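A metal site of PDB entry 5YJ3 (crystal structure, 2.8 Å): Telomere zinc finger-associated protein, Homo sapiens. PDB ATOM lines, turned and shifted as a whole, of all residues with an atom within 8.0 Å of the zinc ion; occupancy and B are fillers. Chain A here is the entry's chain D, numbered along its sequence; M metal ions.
The zinc ion is bound by NE2 of His 59 (2.1 Å). The side-chain sulfur (SG) of Cys 42 is bound to the zinc ion (2.5 Å). A ring nitrogen (NE2) of His 55 binds the zinc ion (2.6 Å).
SG of Cys 42 lies close to SG of Cys 39 (3.6 Å). The side-chain sulfur (SG) of Cys 42 lies close to the backbone NH (N) of Lys 44. The side-chain sulfur (SG) of Cys 39 is in hydrogen-bond range of the backbone NH (N) of Ile 41 (3.6 Å). The side-chain sulfur (SG) of Cys 39 sits at hydrogen-bond distance from the backbone NH (N) of Gly 43, at 3.4 Å. N of Cys 39 lies within hydrogen-bond range of O of Lys 44 (3.1 Å).
Cys 39 touches the zinc ion. Of the 14 residues printed, 4 come within 4 Å of the zinc ion. Along chain A the residues within 4 Å of the zinc ion span positions 39 to 59.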
ATOM      1  N   CYS A  39      21.094  -7.330 -10.627  1.00  0.00           N
ATOM      2  CA  CYS A  39      22.505  -7.505 -10.306  1.00  0.00           C
ATOM      3  C   CYS A  39      22.928  -6.461  -9.273  1.00  0.00           C
ATOM      4  O   CYS A  39      22.098  -5.867  -8.584  1.00  0.00           O
ATOM      5  CB  CYS A  39      23.343  -7.435 -11.589  1.00  0.00           C
ATOM      6  SG  CYS A  39      25.133  -7.302 -11.312  1.00  0.00           S
ATOM      7  N   GLN A  40      24.242  -6.224  -9.161  1.00  0.00           N
ATOM      8  CA  GLN A  40      24.776  -5.236  -8.225  1.00  0.00           C
ATOM      9  C   GLN A  40      25.923  -4.443  -8.840  1.00  0.00           C
ATOM     10  O   GLN A  40      25.824  -3.225  -9.023  1.00  0.00           O
ATOM     11  CB  GLN A  40      25.255  -5.916  -6.942  1.00  0.00           C
ATOM     12  CG  GLN A  40      24.244  -5.880  -5.808  1.00  0.00           C
ATOM     13  CD  GLN A  40      24.911  -5.838  -4.456  1.00  0.00           C
ATOM     14  OE1 GLN A  40      26.035  -5.343  -4.316  1.00  0.00           O
ATOM     15  NE2 GLN A  40      24.238  -6.368  -3.441  1.00  0.00           N
ATOM     16  N   ILE A  41      27.031  -5.125  -9.151  1.00  0.00           N
ATOM     17  CA  ILE A  41      28.241  -4.447  -9.628  1.00  0.00           C
ATOM     18  C   ILE A  41      27.946  -3.677 -10.911  1.00  0.00           C
ATOM     19  O   ILE A  41      28.091  -2.450 -10.957  1.00  0.00           O
ATOM     20  CB  ILE A  41      29.382  -5.455  -9.818  1.00  0.00           C
ATOM     21  N   CYS A  42      27.539  -4.384 -11.958  1.00  0.00           N
ATOM     22  CA  CYS A  42      27.077  -3.696 -13.159  1.00  0.00           C
ATOM     23  C   CYS A  42      25.628  -3.268 -13.007  1.00  0.00           C
ATOM     24  O   CYS A  42      25.297  -2.093 -13.224  1.00  0.00           O
ATOM     25  CB  CYS A  42      27.272  -4.584 -14.393  1.00  0.00           C
ATOM     26  SG  CYS A  42      26.156  -6.000 -14.508  1.00  0.00           S
ATOM     27  N   GLY A  43      24.752  -4.200 -12.636  1.00  0.00           N
ATOM     28  CA  GLY A  43      23.352  -3.896 -12.440  1.00  0.00           C
ATOM     29  C   GLY A  43      22.426  -4.418 -13.515  1.00  0.00           C
ATOM     30  O   GLY A  43      21.333  -3.868 -13.674  1.00  0.00           O
ATOM     31  N   LYS A  44      22.835  -5.450 -14.252  1.00  0.00           N
ATOM     32  CA  LYS A  44      22.013  -5.976 -15.333  1.00  0.00           C
ATOM     33  C   LYS A  44      20.824  -6.756 -14.781  1.00  0.00           C
ATOM     34  O   LYS A  44      20.864  -7.310 -13.679  1.00  0.00           O
ATOM     35  CB  LYS A  44      22.847  -6.874 -16.242  1.00  0.00           C
ATOM     36  N   PHE A  46      18.535  -9.854 -14.375  1.00  0.00           N
ATOM     37  CA  PHE A  46      18.778 -11.283 -14.427  1.00  0.00           C
ATOM     38  C   PHE A  46      17.559 -12.049 -13.930  1.00  0.00           C
ATOM     39  O   PHE A  46      16.867 -11.598 -13.013  1.00  0.00           O
ATOM     40  CB  PHE A  46      20.004 -11.680 -13.612  1.00  0.00           C
ATOM     41  CG  PHE A  46      21.278 -11.679 -14.400  1.00  0.00           C
ATOM     42  CD1 PHE A  46      21.952 -10.506 -14.659  1.00  0.00           C
ATOM     43  CD2 PHE A  46      21.792 -12.867 -14.899  1.00  0.00           C
ATOM     44  CE1 PHE A  46      23.123 -10.506 -15.398  1.00  0.00           C
ATOM     45  CE2 PHE A  46      22.961 -12.874 -15.645  1.00  0.00           C
ATOM     46  CZ  PHE A  46      23.618 -11.685 -15.885  1.00  0.00           C
ATOM     47  N   LEU A  52      23.051 -15.160 -12.358  1.00  0.00           N
ATOM     48  CA  LEU A  52      23.648 -13.964 -11.785  1.00  0.00           C
ATOM     49  C   LEU A  52      24.908 -14.289 -10.986  1.00  0.00           C
ATOM     50  O   LEU A  52      25.847 -13.485 -10.968  1.00  0.00           O
ATOM     51  CB  LEU A  52      22.625 -13.249 -10.904  1.00  0.00           C
ATOM     52  CG  LEU A  52      23.063 -11.904 -10.319  1.00  0.00           C
ATOM     53  CD1 LEU A  52      23.647 -11.011 -11.399  1.00  0.00           C
ATOM     54  CD2 LEU A  52      21.887 -11.221  -9.640  1.00  0.00           C
ATOM     55  N   HIS A  55      27.654 -14.977 -13.423  1.00  0.00           N
ATOM     56  CA  HIS A  55      28.001 -13.690 -14.025  1.00  0.00           C
ATOM     57  C   HIS A  55      28.853 -12.858 -13.083  1.00  0.00           C
ATOM     58  O   HIS A  55      29.757 -12.133 -13.535  1.00  0.00           O
ATOM     59  CB  HIS A  55      26.727 -12.933 -14.412  1.00  0.00           C
ATOM     60  CG  HIS A  55      26.951 -11.483 -14.718  1.00  0.00           C
ATOM     61  ND1 HIS A  55      27.239 -11.033 -15.991  1.00  0.00           N
ATOM     62  CD2 HIS A  55      26.947 -10.389 -13.927  1.00  0.00           C
ATOM     63  CE1 HIS A  55      27.388  -9.724 -15.972  1.00  0.00           C
ATOM     64  NE2 HIS A  55      27.216  -9.302 -14.726  1.00  0.00           N
ATOM     65  N   VAL A  56      28.579 -12.924 -11.780  1.00  0.00           N
ATOM     66  CA  VAL A  56      29.418 -12.225 -10.819  1.00  0.00           C
ATOM     67  C   VAL A  56      30.815 -12.828 -10.785  1.00  0.00           C
ATOM     68  O   VAL A  56      31.790 -12.128 -10.483  1.00  0.00           O
ATOM     69  CB  VAL A  56      28.773 -12.238  -9.421  1.00  0.00           C
ATOM     70  N   ARG A  57      30.941 -14.126 -11.092  1.00  0.00           N
ATOM     71  CA  ARG A  57      32.254 -14.759 -11.086  1.00  0.00           C
ATOM     72  C   ARG A  57      33.209 -14.107 -12.080  1.00  0.00           C
ATOM     73  O   ARG A  57      34.405 -13.964 -11.800  1.00  0.00           O
ATOM     74  CB  ARG A  57      32.114 -16.256 -11.368  1.00  0.00           C
ATOM     75  N   ARG A  58      32.705 -13.694 -13.244  1.00  0.00           N
ATOM     76  CA  ARG A  58      33.525 -13.153 -14.331  1.00  0.00           C
ATOM     77  C   ARG A  58      33.226 -11.673 -14.486  1.00  0.00           C
ATOM     78  O   ARG A  58      32.219 -11.291 -15.097  1.00  0.00           O
ATOM     79  CB  ARG A  58      33.275 -13.915 -15.625  1.00  0.00           C
ATOM     80  N   HIS A  59      34.110 -10.815 -13.962  1.00  0.00           N
ATOM     81  CA  HIS A  59      33.908  -9.378 -14.075  1.00  0.00           C
ATOM     82  C   HIS A  59      35.202  -8.584 -14.182  1.00  0.00           C
ATOM     83  O   HIS A  59      35.170  -7.362 -14.018  1.00  0.00           O
ATOM     84  CB  HIS A  59      33.083  -8.864 -12.885  1.00  0.00           C
ATOM     85  CG  HIS A  59      31.851  -8.097 -13.280  1.00  0.00           C
ATOM     86  ND1 HIS A  59      31.904  -6.951 -14.054  1.00  0.00           N
ATOM     87  CD2 HIS A  59      30.542  -8.305 -13.004  1.00  0.00           C
ATOM     88  CE1 HIS A  59      30.680  -6.488 -14.232  1.00  0.00           C
ATOM     89  NE2 HIS A  59      29.840  -7.298 -13.613  1.00  0.00           N
ATOM     90  N   VAL A  62      37.273  -5.578 -10.502  1.00  0.00           N
ATOM     91  CA  VAL A  62      36.402  -5.040  -9.462  1.00  0.00           C
ATOM     92  C   VAL A  62      37.302  -4.428  -8.398  1.00  0.00           C
ATOM     93  O   VAL A  62      37.901  -5.146  -7.591  1.00  0.00           O
ATOM     94  CB  VAL A  62      35.481  -6.112  -8.883  1.00  0.00           C
ATOM     95  CG1 VAL A  62      34.691  -5.560  -7.695  1.00  0.00           C
ATOM     96  CG2 VAL A  62      34.533  -6.630  -9.954  1.00  0.00           C
HETATM   97 ZN    ZN M   1      27.780  -7.347 -13.108  1.00  0.00          ZN
